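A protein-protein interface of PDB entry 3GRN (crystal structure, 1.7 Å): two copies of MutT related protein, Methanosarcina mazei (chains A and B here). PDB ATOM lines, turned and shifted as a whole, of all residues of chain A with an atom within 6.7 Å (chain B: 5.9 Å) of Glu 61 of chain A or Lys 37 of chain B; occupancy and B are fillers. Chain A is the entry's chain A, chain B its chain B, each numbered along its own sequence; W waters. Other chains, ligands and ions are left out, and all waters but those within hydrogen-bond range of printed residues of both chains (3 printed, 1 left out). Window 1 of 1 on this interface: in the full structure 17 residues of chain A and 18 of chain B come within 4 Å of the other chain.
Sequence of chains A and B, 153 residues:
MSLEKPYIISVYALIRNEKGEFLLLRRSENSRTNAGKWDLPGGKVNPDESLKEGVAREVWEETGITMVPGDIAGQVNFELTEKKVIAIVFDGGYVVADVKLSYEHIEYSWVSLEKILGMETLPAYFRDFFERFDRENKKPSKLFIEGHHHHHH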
ATOM      1  N   ASN A  46      -8.016 -23.894 -20.524  1.00  0.00           N
ATOM      2  CA  ASN A  46      -8.847 -22.821 -19.952  1.00  0.00           C
ATOM      3  C   ASN A  46     -10.165 -22.711 -20.689  1.00  0.00           C
ATOM      4  O   ASN A  46     -10.272 -23.197 -21.831  1.00  0.00           O
ATOM      5  CB  ASN A  46      -8.130 -21.456 -19.999  1.00  0.00           C
ATOM      6  CG  ASN A  46      -7.112 -21.271 -18.896  1.00  0.00           C
ATOM      7  OD1 ASN A  46      -7.146 -21.934 -17.852  1.00  0.00           O
ATOM      8  ND2 ASN A  46      -6.168 -20.368 -19.132  1.00  0.00           N
ATOM      9  N   ALA A  56       0.945 -24.660 -25.339  1.00  0.00           N
ATOM     10  CA  ALA A  56       2.052 -23.684 -25.405  1.00  0.00           C
ATOM     11  C   ALA A  56       2.090 -22.792 -24.140  1.00  0.00           C
ATOM     12  O   ALA A  56       3.161 -22.548 -23.594  1.00  0.00           O
ATOM     13  CB  ALA A  56       1.975 -22.850 -26.674  1.00  0.00           C
ATOM     14  N   ARG A  57       0.910 -22.364 -23.681  1.00  0.00           N
ATOM     15  CA  ARG A  57       0.748 -21.544 -22.467  1.00  0.00           C
ATOM     16  C   ARG A  57       1.257 -22.292 -21.247  1.00  0.00           C
ATOM     17  O   ARG A  57       2.046 -21.761 -20.480  1.00  0.00           O
ATOM     18  CB  ARG A  57      -0.728 -21.185 -22.272  1.00  0.00           C
ATOM     19  CG  ARG A  57      -1.001 -20.420 -20.978  1.00  0.00           C
ATOM     20  CD  ARG A  57      -2.496 -20.213 -20.722  1.00  0.00           C
ATOM     21  NE  ARG A  57      -3.301 -21.443 -20.785  1.00  0.00           N
ATOM     22  CZ  ARG A  57      -3.459 -22.328 -19.813  1.00  0.00           C
ATOM     23  NH1 ARG A  57      -2.843 -22.206 -18.636  1.00  0.00           N
ATOM     24  NH2 ARG A  57      -4.244 -23.381 -20.034  1.00  0.00           N
ATOM     25  N   GLU A  58       0.819 -23.543 -21.083  1.00  0.00           N
ATOM     26  CA  GLU A  58       1.261 -24.371 -19.946  1.00  0.00           C
ATOM     27  C   GLU A  58       2.763 -24.648 -19.950  1.00  0.00           C
ATOM     28  O   GLU A  58       3.413 -24.585 -18.906  1.00  0.00           O
ATOM     29  CB  GLU A  58       0.467 -25.669 -19.923  1.00  0.00           C
ATOM     30  CG  GLU A  58      -0.995 -25.409 -19.549  1.00  0.00           C
ATOM     31  CD  GLU A  58      -1.265 -25.217 -18.054  1.00  0.00           C
ATOM     32  OE1 GLU A  58      -0.337 -25.328 -17.229  1.00  0.00           O
ATOM     33  OE2 GLU A  58      -2.445 -24.962 -17.705  1.00  0.00           O
ATOM     34  N   VAL A  59       3.305 -24.956 -21.111  1.00  0.00           N
ATOM     35  CA  VAL A  59       4.735 -25.217 -21.231  1.00  0.00           C
ATOM     36  C   VAL A  59       5.542 -23.961 -20.891  1.00  0.00           C
ATOM     37  O   VAL A  59       6.476 -24.053 -20.098  1.00  0.00           O
ATOM     38  CB  VAL A  59       5.084 -25.762 -22.598  1.00  0.00           C
ATOM     39  CG1 VAL A  59       6.586 -25.720 -22.825  1.00  0.00           C
ATOM     40  CG2 VAL A  59       4.563 -27.189 -22.680  1.00  0.00           C
ATOM     41  N   TRP A  60       5.138 -22.805 -21.428  1.00  0.00           N
ATOM     42  CA  TRP A  60       5.846 -21.555 -21.097  1.00  0.00           C
ATOM     43  C   TRP A  60       5.819 -21.251 -19.603  1.00  0.00           C
ATOM     44  O   TRP A  60       6.871 -21.002 -19.007  1.00  0.00           O
ATOM     45  CB  TRP A  60       5.414 -20.324 -21.881  1.00  0.00           C
ATOM     46  CG  TRP A  60       6.504 -19.256 -21.670  1.00  0.00           C
ATOM     47  CD1 TRP A  60       7.757 -19.224 -22.259  1.00  0.00           C
ATOM     48  CD2 TRP A  60       6.481 -18.172 -20.740  1.00  0.00           C
ATOM     49  NE1 TRP A  60       8.485 -18.156 -21.772  1.00  0.00           N
ATOM     50  CE2 TRP A  60       7.728 -17.497 -20.844  1.00  0.00           C
ATOM     51  CE3 TRP A  60       5.525 -17.687 -19.837  1.00  0.00           C
ATOM     52  CZ2 TRP A  60       8.031 -16.362 -20.095  1.00  0.00           C
ATOM     53  CZ3 TRP A  60       5.843 -16.559 -19.085  1.00  0.00           C
ATOM     54  CH2 TRP A  60       7.079 -15.911 -19.222  1.00  0.00           C
ATOM     55  N   GLU A  61       4.640 -21.348 -18.979  1.00  0.00           N
ATOM     56  CA  GLU A  61       4.514 -20.972 -17.572  1.00  0.00           C
ATOM     57  C   GLU A  61       5.237 -21.926 -16.644  1.00  0.00           C
ATOM     58  O   GLU A  61       5.735 -21.509 -15.611  1.00  0.00           O
ATOM     59  CB  GLU A  61       3.047 -20.847 -17.163  1.00  0.00           C
ATOM     60  CG  GLU A  61       2.345 -19.729 -17.890  1.00  0.00           C
ATOM     61  CD  GLU A  61       0.970 -19.423 -17.326  1.00  0.00           C
ATOM     62  OE1 GLU A  61       0.509 -20.155 -16.407  1.00  0.00           O
ATOM     63  OE2 GLU A  61       0.359 -18.448 -17.824  1.00  0.00           O
ATOM     64  N   GLU A  62       5.347 -23.203 -17.045  1.00  0.00           N
ATOM     65  CA  GLU A  62       5.953 -24.199 -16.164  1.00  0.00           C
ATOM     66  C   GLU A  62       7.459 -24.341 -16.317  1.00  0.00           C
ATOM     67  O   GLU A  62       8.140 -24.815 -15.403  1.00  0.00           O
ATOM     68  CB  GLU A  62       5.300 -25.552 -16.387  1.00  0.00           C
ATOM     69  CG  GLU A  62       3.822 -25.513 -15.985  1.00  0.00           C
ATOM     70  CD  GLU A  62       3.108 -26.804 -16.177  1.00  0.00           C
ATOM     71  OE1 GLU A  62       3.662 -27.712 -16.818  1.00  0.00           O
ATOM     72  OE2 GLU A  62       1.971 -26.891 -15.680  1.00  0.00           O
ATOM     73  N   THR A  63       7.960 -24.002 -17.509  1.00  0.00           N
ATOM     74  CA  THR A  63       9.354 -24.321 -17.852  1.00  0.00           C
ATOM     75  C   THR A  63      10.136 -23.171 -18.499  1.00  0.00           C
ATOM     76  O   THR A  63      11.351 -23.272 -18.633  1.00  0.00           O
ATOM     77  CB  THR A  63       9.460 -25.508 -18.846  1.00  0.00           C
ATOM     78  OG1 THR A  63       9.042 -25.080 -20.143  1.00  0.00           O
ATOM     79  CG2 THR A  63       8.653 -26.780 -18.395  1.00  0.00           C
ATOM     80  N   GLY A  64       9.466 -22.110 -18.940  1.00  0.00           N
ATOM     81  CA  GLY A  64      10.180 -21.016 -19.642  1.00  0.00           C
ATOM     82  C   GLY A  64      10.383 -21.288 -21.135  1.00  0.00           C
ATOM     83  O   GLY A  64      10.909 -20.432 -21.864  1.00  0.00           O
ATOM     84  N   ILE A  65       9.996 -22.481 -21.590  1.00  0.00           N
ATOM     85  CA  ILE A  65      10.166 -22.876 -22.989  1.00  0.00           C
ATOM     86  C   ILE A  65       9.074 -22.305 -23.873  1.00  0.00           C
ATOM     87  O   ILE A  65       7.884 -22.456 -23.586  1.00  0.00           O
ATOM     88  CB  ILE A  65      10.260 -24.428 -23.144  1.00  0.00           C
ATOM     89  CG1 ILE A  65      11.500 -24.945 -22.392  1.00  0.00           C
ATOM     90  CG2 ILE A  65      10.301 -24.870 -24.646  1.00  0.00           C
ATOM     91  CD1 ILE A  65      11.548 -26.431 -22.191  1.00  0.00           C
ATOM     92  N   LYS A 100      13.373 -23.519 -16.523  1.00  0.00           N
ATOM     93  CA  LYS A 100      13.200 -22.602 -15.438  1.00  0.00           C
ATOM     94  C   LYS A 100      11.816 -22.810 -14.837  1.00  0.00           C
ATOM     95  O   LYS A 100      10.799 -22.534 -15.476  1.00  0.00           O
ATOM     96  CB  LYS A 100      13.390 -21.166 -15.926  1.00  0.00           C
ATOM     97  CG  LYS A 100      14.859 -20.869 -16.335  1.00  0.00           C
ATOM     98  CD  LYS A 100      15.081 -19.386 -16.616  1.00  0.00           C
ATOM     99  CE  LYS A 100      16.580 -19.047 -16.698  1.00  0.00           C
ATOM    100  NZ  LYS A 100      17.311 -19.825 -17.753  1.00  0.00           N
ATOM    101  N   LEU A 101      11.804 -23.281 -13.602  1.00  0.00           N
ATOM    102  CA  LEU A 101      10.561 -23.748 -12.938  1.00  0.00           C
ATOM    103  C   LEU A 101       9.765 -22.680 -12.231  1.00  0.00           C
ATOM    104  O   LEU A 101      10.285 -21.605 -11.922  1.00  0.00           O
ATOM    105  CB  LEU A 101      10.892 -24.850 -11.923  1.00  0.00           C
ATOM    106  CG  LEU A 101      11.521 -26.123 -12.524  1.00  0.00           C
ATOM    107  CD1 LEU A 101      11.805 -27.114 -11.430  1.00  0.00           C
ATOM    108  CD2 LEU A 101      10.623 -26.717 -13.584  1.00  0.00           C
ATOM    109  N   SER A 102       8.503 -23.006 -11.956  1.00  0.00           N
ATOM    110  CA  SER A 102       7.582 -22.152 -11.227  1.00  0.00           C
ATOM    111  C   SER A 102       7.226 -22.821  -9.890  1.00  0.00           C
ATOM    112  O   SER A 102       7.696 -23.949  -9.602  1.00  0.00           O
ATOM    113  CB  SER A 102       6.310 -21.964 -12.040  1.00  0.00           C
ATOM    114  OG  SER A 102       5.517 -23.158 -11.965  1.00  0.00           O
ATOM    115  N   TYR A 103       6.360 -22.152  -9.112  1.00  0.00           N
ATOM    116  CA  TYR A 103       5.840 -22.696  -7.846  1.00  0.00           C
ATOM    117  C   TYR A 103       5.226 -24.086  -7.994  1.00  0.00           C
ATOM    118  O   TYR A 103       5.134 -24.822  -7.010  1.00  0.00           O
ATOM    119  CB  TYR A 103       4.775 -21.749  -7.254  1.00  0.00           C
ATOM    120  CG  TYR A 103       3.503 -21.591  -8.070  1.00  0.00           C
ATOM    121  CD1 TYR A 103       2.326 -22.291  -7.724  1.00  0.00           C
ATOM    122  CD2 TYR A 103       3.436 -20.688  -9.133  1.00  0.00           C
ATOM    123  CE1 TYR A 103       1.138 -22.121  -8.449  1.00  0.00           C
ATOM    124  CE2 TYR A 103       2.246 -20.508  -9.867  1.00  0.00           C
ATOM    125  CZ  TYR A 103       1.108 -21.234  -9.525  1.00  0.00           C
ATOM    126  OH  TYR A 103      -0.061 -21.060 -10.250  1.00  0.00           O
ATOM    127  N   GLU A 104       4.813 -24.438  -9.215  1.00  0.00           N
ATOM    128  CA  GLU A 104       4.108 -25.709  -9.454  1.00  0.00           C
ATOM    129  C   GLU A 104       5.015 -26.932  -9.348  1.00  0.00           C
ATOM    130  O   GLU A 104       4.535 -28.047  -9.117  1.00  0.00           O
ATOM    131  CB  GLU A 104       3.379 -25.681 -10.808  1.00  0.00           C
ATOM    132  CG  GLU A 104       2.254 -24.640 -10.877  1.00  0.00           C
ATOM    133  CD  GLU A 104       1.300 -24.850 -12.050  1.00  0.00           C
ATOM    134  OE1 GLU A 104       1.776 -25.067 -13.191  1.00  0.00           O
ATOM    135  OE2 GLU A 104       0.068 -24.783 -11.827  1.00  0.00           O
ATOM    136  N   LEU B  25     -10.353 -11.983  -8.878  1.00  0.00           N
ATOM    137  CA  LEU B  25     -10.419 -11.623 -10.291  1.00  0.00           C
ATOM    138  C   LEU B  25      -9.753 -12.724 -11.114  1.00  0.00           C
ATOM    139  O   LEU B  25      -8.733 -13.255 -10.691  1.00  0.00           O
ATOM    140  CB  LEU B  25      -9.620 -10.342 -10.504  1.00  0.00           C
ATOM    141  CG  LEU B  25      -9.853  -9.157  -9.561  1.00  0.00           C
ATOM    142  CD1 LEU B  25      -8.848  -8.042  -9.943  1.00  0.00           C
ATOM    143  CD2 LEU B  25     -11.303  -8.686  -9.664  1.00  0.00           C
ATOM    144  N   ARG B  26     -10.324 -13.067 -12.272  1.00  0.00           N
ATOM    145  CA  ARG B  26      -9.711 -14.098 -13.122  1.00  0.00           C
ATOM    146  C   ARG B  26      -8.908 -13.435 -14.217  1.00  0.00           C
ATOM    147  O   ARG B  26      -9.441 -12.610 -14.945  1.00  0.00           O
ATOM    148  CB  ARG B  26     -10.770 -15.003 -13.747  1.00  0.00           C
ATOM    149  CG  ARG B  26     -10.126 -16.198 -14.459  1.00  0.00           C
ATOM    150  CD  ARG B  26     -11.090 -17.334 -14.711  1.00  0.00           C
ATOM    151  NE  ARG B  26     -11.888 -17.148 -15.918  1.00  0.00           N
ATOM    152  CZ  ARG B  26     -11.486 -17.415 -17.168  1.00  0.00           C
ATOM    153  NH1 ARG B  26     -12.325 -17.214 -18.174  1.00  0.00           N
ATOM    154  NH2 ARG B  26     -10.253 -17.855 -17.438  1.00  0.00           N
ATOM    155  N   ARG B  27      -7.644 -13.809 -14.341  1.00  0.00           N
ATOM    156  CA  ARG B  27      -6.682 -13.158 -15.225  1.00  0.00           C
ATOM    157  C   ARG B  27      -6.984 -13.443 -16.698  1.00  0.00           C
ATOM    158  O   ARG B  27      -7.511 -14.510 -17.008  1.00  0.00           O
ATOM    159  CB  ARG B  27      -5.275 -13.636 -14.890  1.00  0.00           C
ATOM    160  CG  ARG B  27      -4.830 -13.253 -13.472  1.00  0.00           C
ATOM    161  CD  ARG B  27      -3.478 -13.888 -13.100  1.00  0.00           C
ATOM    162  NE  ARG B  27      -2.354 -13.407 -13.914  1.00  0.00           N
ATOM    163  CZ  ARG B  27      -1.733 -12.239 -13.739  1.00  0.00           C
ATOM    164  NH1 ARG B  27      -2.124 -11.405 -12.785  1.00  0.00           N
ATOM    165  NH2 ARG B  27      -0.720 -11.894 -14.526  1.00  0.00           N
ATOM    166  N   SER B  28      -6.634 -12.498 -17.575  1.00  0.00           N
ATOM    167  CA  SER B  28      -6.886 -12.653 -19.006  1.00  0.00           C
ATOM    168  C   SER B  28      -5.952 -13.700 -19.616  1.00  0.00           C
ATOM    169  O   SER B  28      -4.855 -13.957 -19.087  1.00  0.00           O
ATOM    170  CB  SER B  28      -6.764 -11.330 -19.741  1.00  0.00           C
ATOM    171  OG  SER B  28      -5.463 -10.805 -19.592  1.00  0.00           O
ATOM    172  N   SER B  31      -2.243 -12.764 -20.630  1.00  0.00           N
ATOM    173  CA  SER B  31      -1.262 -12.494 -19.581  1.00  0.00           C
ATOM    174  C   SER B  31      -0.030 -13.386 -19.719  1.00  0.00           C
ATOM    175  O   SER B  31      -0.130 -14.578 -20.035  1.00  0.00           O
ATOM    176  CB  SER B  31      -1.879 -12.709 -18.195  1.00  0.00           C
ATOM    177  OG  SER B  31      -3.108 -12.013 -18.060  1.00  0.00           O
ATOM    178  N   ARG B  32       1.125 -12.790 -19.455  1.00  0.00           N
ATOM    179  CA  ARG B  32       2.407 -13.486 -19.497  1.00  0.00           C
ATOM    180  C   ARG B  32       2.582 -14.489 -18.339  1.00  0.00           C
ATOM    181  O   ARG B  32       3.270 -15.498 -18.484  1.00  0.00           O
ATOM    182  CB  ARG B  32       3.531 -12.447 -19.500  1.00  0.00           C
ATOM    183  CG  ARG B  32       4.906 -12.993 -19.779  1.00  0.00           C
ATOM    184  CD  ARG B  32       5.960 -11.940 -19.483  1.00  0.00           C
ATOM    185  NE  ARG B  32       7.313 -12.374 -19.831  1.00  0.00           N
ATOM    186  CZ  ARG B  32       7.823 -12.353 -21.064  1.00  0.00           C
ATOM    187  NH1 ARG B  32       7.095 -11.924 -22.091  1.00  0.00           N
ATOM    188  NH2 ARG B  32       9.067 -12.769 -21.273  1.00  0.00           N
ATOM    189  N   THR B  33       1.959 -14.210 -17.193  1.00  0.00           N
ATOM    190  CA  THR B  33       2.041 -15.093 -16.026  1.00  0.00           C
ATOM    191  C   THR B  33       0.634 -15.496 -15.595  1.00  0.00           C
ATOM    192  O   THR B  33      -0.296 -14.667 -15.614  1.00  0.00           O
ATOM    193  CB  THR B  33       2.777 -14.422 -14.821  1.00  0.00           C
ATOM    194  OG1 THR B  33       1.966 -13.372 -14.276  1.00  0.00           O
ATOM    195  CG2 THR B  33       4.122 -13.832 -15.243  1.00  0.00           C
ATOM    196  N   ASN B  34       0.470 -16.765 -15.226  1.00  0.00           N
ATOM    197  CA  ASN B  34      -0.797 -17.289 -14.666  1.00  0.00           C
ATOM    198  C   ASN B  34      -2.022 -16.917 -15.486  1.00  0.00           C
ATOM    199  O   ASN B  34      -3.076 -16.585 -14.924  1.00  0.00           O
ATOM    200  CB  ASN B  34      -1.009 -16.812 -13.210  1.00  0.00           C
ATOM    201  CG  ASN B  34      -0.149 -17.560 -12.201  1.00  0.00           C
ATOM    202  OD1 ASN B  34       0.567 -16.942 -11.406  1.00  0.00           O
ATOM    203  ND2 ASN B  34      -0.233 -18.889 -12.208  1.00  0.00           N
ATOM    204  N   ALA B  35      -1.884 -16.974 -16.815  1.00  0.00           N
ATOM    205  CA  ALA B  35      -2.962 -16.604 -17.717  1.00  0.00           C
ATOM    206  C   ALA B  35      -4.214 -17.443 -17.422  1.00  0.00           C
ATOM    207  O   ALA B  35      -4.134 -18.638 -17.177  1.00  0.00           O
ATOM    208  CB  ALA B  35      -2.519 -16.768 -19.163  1.00  0.00           C
ATOM    209  N   GLY B  36      -5.358 -16.791 -17.329  1.00  0.00           N
ATOM    210  CA  GLY B  36      -6.595 -17.525 -17.102  1.00  0.00           C
ATOM    211  C   GLY B  36      -6.917 -17.944 -15.686  1.00  0.00           C
ATOM    212  O   GLY B  36      -8.006 -18.479 -15.444  1.00  0.00           O
ATOM    213  N   LYS B  37      -5.997 -17.702 -14.743  1.00  0.00           N
ATOM    214  CA  LYS B  37      -6.182 -18.135 -13.348  1.00  0.00           C
ATOM    215  C   LYS B  37      -6.819 -17.058 -12.442  1.00  0.00           C
ATOM    216  O   LYS B  37      -6.717 -15.866 -12.732  1.00  0.00           O
ATOM    217  CB  LYS B  37      -4.844 -18.582 -12.754  1.00  0.00           C
ATOM    218  CG  LYS B  37      -4.207 -19.767 -13.480  1.00  0.00           C
ATOM    219  CD  LYS B  37      -3.349 -20.595 -12.529  1.00  0.00           C
ATOM    220  CE  LYS B  37      -2.992 -21.963 -13.121  1.00  0.00           C
ATOM    221  NZ  LYS B  37      -2.005 -21.879 -14.244  1.00  0.00           N
ATOM    222  N   TRP B  38      -7.461 -17.493 -11.357  1.00  0.00           N
ATOM    223  CA  TRP B  38      -7.976 -16.576 -10.313  1.00  0.00           C
ATOM    224  C   TRP B  38      -6.849 -15.903  -9.509  1.00  0.00           C
ATOM    225  O   TRP B  38      -5.782 -16.476  -9.333  1.00  0.00           O
ATOM    226  CB  TRP B  38      -8.967 -17.287  -9.391  1.00  0.00           C
ATOM    227  CG  TRP B  38     -10.222 -17.622 -10.121  1.00  0.00           C
ATOM    228  CD1 TRP B  38     -10.507 -18.791 -10.781  1.00  0.00           C
ATOM    229  CD2 TRP B  38     -11.333 -16.756 -10.335  1.00  0.00           C
ATOM    230  NE1 TRP B  38     -11.753 -18.709 -11.366  1.00  0.00           N
ATOM    231  CE2 TRP B  38     -12.281 -17.469 -11.105  1.00  0.00           C
ATOM    232  CE3 TRP B  38     -11.638 -15.449  -9.931  1.00  0.00           C
ATOM    233  CZ2 TRP B  38     -13.514 -16.910 -11.482  1.00  0.00           C
ATOM    234  CZ3 TRP B  38     -12.852 -14.900 -10.303  1.00  0.00           C
ATOM    235  CH2 TRP B  38     -13.777 -15.631 -11.071  1.00  0.00           C
ATOM    236  N   ASP B  39      -7.086 -14.672  -9.047  1.00  0.00           N
ATOM    237  CA  ASP B  39      -6.021 -13.837  -8.482  1.00  0.00           C
ATOM    238  C   ASP B  39      -6.669 -12.852  -7.517  1.00  0.00           C
ATOM    239  O   ASP B  39      -7.884 -12.674  -7.550  1.00  0.00           O
ATOM    240  CB  ASP B  39      -5.341 -13.063  -9.625  1.00  0.00           C
ATOM    241  CG  ASP B  39      -3.902 -12.687  -9.318  1.00  0.00           C
ATOM    242  OD1 ASP B  39      -3.464 -12.863  -8.172  1.00  0.00           O
ATOM    243  OD2 ASP B  39      -3.199 -12.215 -10.234  1.00  0.00           O
ATOM    244  N   LEU B  80       7.907 -17.796 -10.037  1.00  0.00           N
ATOM    245  CA  LEU B  80       7.392 -17.915 -11.399  1.00  0.00           C
ATOM    246  C   LEU B  80       8.586 -18.272 -12.255  1.00  0.00           C
ATOM    247  O   LEU B  80       9.724 -18.267 -11.768  1.00  0.00           O
ATOM    248  CB  LEU B  80       6.771 -16.610 -11.859  1.00  0.00           C
ATOM    249  CG  LEU B  80       5.549 -16.102 -11.085  1.00  0.00           C
ATOM    250  CD1 LEU B  80       5.135 -14.736 -11.613  1.00  0.00           C
ATOM    251  CD2 LEU B  80       4.410 -17.111 -11.173  1.00  0.00           C
ATOM    252  N   THR B  81       8.351 -18.592 -13.525  1.00  0.00           N
ATOM    253  CA  THR B  81       9.457 -18.997 -14.351  1.00  0.00           C
ATOM    254  C   THR B  81      10.544 -17.923 -14.508  1.00  0.00           C
ATOM    255  O   THR B  81      11.724 -18.275 -14.463  1.00  0.00           O
ATOM    256  CB  THR B  81       8.982 -19.580 -15.721  1.00  0.00           C
ATOM    257  OG1 THR B  81      10.134 -20.018 -16.447  1.00  0.00           O
ATOM    258  CG2 THR B  81       8.248 -18.518 -16.519  1.00  0.00           C
ATOM    259  N   HIS B 105      -8.094  -8.593 -16.666  1.00  0.00           N
ATOM    260  CA  HIS B 105      -8.961  -9.618 -16.113  1.00  0.00           C
ATOM    261  C   HIS B 105     -10.258  -9.812 -16.889  1.00  0.00           C
ATOM    262  O   HIS B 105     -10.782  -8.852 -17.466  1.00  0.00           O
ATOM    263  CB  HIS B 105      -9.309  -9.335 -14.647  1.00  0.00           C
ATOM    264  CG  HIS B 105      -8.124  -9.219 -13.751  1.00  0.00           C
ATOM    265  ND1 HIS B 105      -7.522  -8.011 -13.471  1.00  0.00           N
ATOM    266  CD2 HIS B 105      -7.419 -10.162 -13.082  1.00  0.00           C
ATOM    267  CE1 HIS B 105      -6.505  -8.214 -12.649  1.00  0.00           C
ATOM    268  NE2 HIS B 105      -6.417  -9.511 -12.407  1.00  0.00           N
ATOM    269  N   THR B 121      -8.525 -23.669  -8.641  1.00  0.00           N
ATOM    270  CA  THR B 121      -8.007 -22.812  -9.702  1.00  0.00           C
ATOM    271  C   THR B 121      -7.478 -21.498  -9.138  1.00  0.00           C
ATOM    272  O   THR B 121      -6.829 -20.725  -9.843  1.00  0.00           O
ATOM    273  CB  THR B 121      -9.085 -22.510 -10.759  1.00  0.00           C
ATOM    274  OG1 THR B 121     -10.385 -22.638 -10.172  1.00  0.00           O
ATOM    275  CG2 THR B 121      -8.966 -23.474 -11.930  1.00  0.00           C
ATOM    276  N   PRO B 123      -4.537 -20.333  -7.119  1.00  0.00           N
ATOM    277  CA  PRO B 123      -3.219 -20.925  -6.960  1.00  0.00           C
ATOM    278  C   PRO B 123      -2.877 -21.246  -5.517  1.00  0.00           C
ATOM    279  O   PRO B 123      -3.296 -20.518  -4.599  1.00  0.00           O
ATOM    280  CB  PRO B 123      -2.288 -19.833  -7.486  1.00  0.00           C
ATOM    281  CG  PRO B 123      -3.103 -19.066  -8.425  1.00  0.00           C
ATOM    282  CD  PRO B 123      -4.456 -19.028  -7.804  1.00  0.00           C
HETATM  283  O   HOH W   1      -2.040 -20.327 -16.491  1.00  0.00           O
HETATM  284  O   HOH W   2      -4.377 -21.790 -16.211  1.00  0.00           O
HETATM  285  O   HOH W   3       5.530 -19.088 -14.274  1.00  0.00           O
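The backbone carbonyl oxygen of Ala 35 of chain B lies within hydrogen-bond range of the side-chain amide nitrogen of Asn 46 of chain A (3.3 Å). N of Asn 34 of chain B sits at hydrogen-bond distance from OE2 of Glu 61 of chain A. The backbone NH (N) of Ala 35 of chain B is in hydrogen-bond range of the side-chain carboxylate (OE2) of Glu 61 of chain A, at 2.9 Å. The side-chain carboxylate (OE1) of Glu 61 of chain A lies within salt-bridge range of the side-chain amino group (NZ) of Lys 37 of chain B. N of Gly 64 of chain A sits at hydrogen-bond distance from OG1 of Thr 81 of chain B. OG1 of Thr 81 of chain B sits at hydrogen-bond distance from O of Lys 100 of chain A. The side-chain amide nitrogen (ND2) of Asn 34 of chain B lies within hydrogen-bond range of the side-chain hydroxyl (OH) of Tyr 103 of chain A (2.9 Å). O of Leu 101 of chain A lies close to O of Leu 80 of chain B (3.4 Å).
NE of Arg 57 of chain A lies close to ND2 of Asn 46 of chain A (3.5 Å). The backbone carbonyl oxygen (O) of Thr 63 of chain A sits at hydrogen-bond distance from the backbone NH (N) of Lys 100 of chain A (2.9 Å). O of Asn 34 of chain B lies close to NE of Arg 27 of chain B, at 3.4 Å. The backbone carbonyl oxygen (O) of Arg 27 of chain B lies close to the backbone NH (N) of Gly 36 of chain B, 3.2 Å away. The backbone NH (N) of Arg 27 of chain B sits at hydrogen-bond distance from the backbone carbonyl oxygen (O) of Lys 37 of chain B (2.8 Å). N of Gly 36 of chain B sits at hydrogen-bond distance from O of Ser 28 of chain B (3.4 Å).
Asn 46 of chain A touches Gly 36 of chain B (ND2 to CA, 3.5 Å). CD of Arg 57 of chain A touches CB of Ala 35 of chain B, 3.8 Å away. Arg 32 of chain B touches Trp 60 of chain A. CG2 of Thr 81 of chain B touches O of Trp 60 of chain A, 3.8 Å away. OE2 of Glu 61 of chain A touches C of Thr 33 of chain B (3.7 Å). Thr 81 of chain B touches Glu 61 of chain A (CB to O, 3.8 Å). Thr 81 of chain B touches Thr 63 of chain A. Leu 101 of chain A touches Thr 81 of chain B. Pro 123 of chain B touches Tyr 103 of chain A (CB to OH, 3.8 Å).
Printed residues of chain B within 4 Å of Asn 46 of chain A: Ala 35 and Gly 36. Printed residues of chain B within 4 Å of Arg 57 of chain A: Ala 35 (3.8 Å). Of chain B, only Thr 33 (3.7 Å), Asn 34 (3.1 Å), Ala 35 (2.9 Å), Lys 37 (3.7 Å) and Thr 81 (3.8 Å) come within 4 Å of Glu 61 of chain A. Of the printed residues of chain A, Arg 32 of chain B touches Trp 60 (2.8 Å). Lys 37 of chain B touches just one residue of chain A: Glu 61. The nearest residue of chain A that does not touch Lys 37 of chain B is Tyr 103 of chain A (4.03 Å).
Printed residues of chain B that touch a printed residue of chain A: Arg 32, Thr 33, Asn 34, Ala 35, Gly 36, Lys 37, Leu 80, Thr 81 and Pro 123. Hydrophobic or aromatic side chains of chain B within 4 Å of the printed part of chain A: Ala 35 and Pro 123. Along chain A the printed residues that touch a printed residue of chain B span positions 46 to 103. Among the printed residues, Asp or Glu carboxylates within 4 Å of a Lys or Arg side-chain nitrogen of the other chain: Glu 61 of chain A with Lys 37 of chain B.
No position is printed for both chains. Of the 17 pairs that touch across the chains among the printed residues, none has its exchanged pair printed and touching as well.
Water W1 lies within hydrogen-bond range of OE1 of Glu 61 of chain A, NZ of Lys 37 of chain B, O of Ala 35 of chain B and NH1 of Arg 57 of chain A. Water W3 bridges the backbone carbonyl oxygen (O) of Glu 61 of chain A (2.8 Å) and the backbone NH (N) of Thr 81 of chain B (3.0 Å). Water W2 lies within hydrogen-bond range of the guanidinium group (NH1) of Arg 57 of chain A (2.9 Å), the side-chain amino group (NZ) of Lys 37 of chain B (3.1 Å), the side-chain amide oxygen (OD1) of Asn 46 of chain A (3.2 Å) and the backbone carbonyl oxygen (O) of Ala 35 of chain B (3.3 Å).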
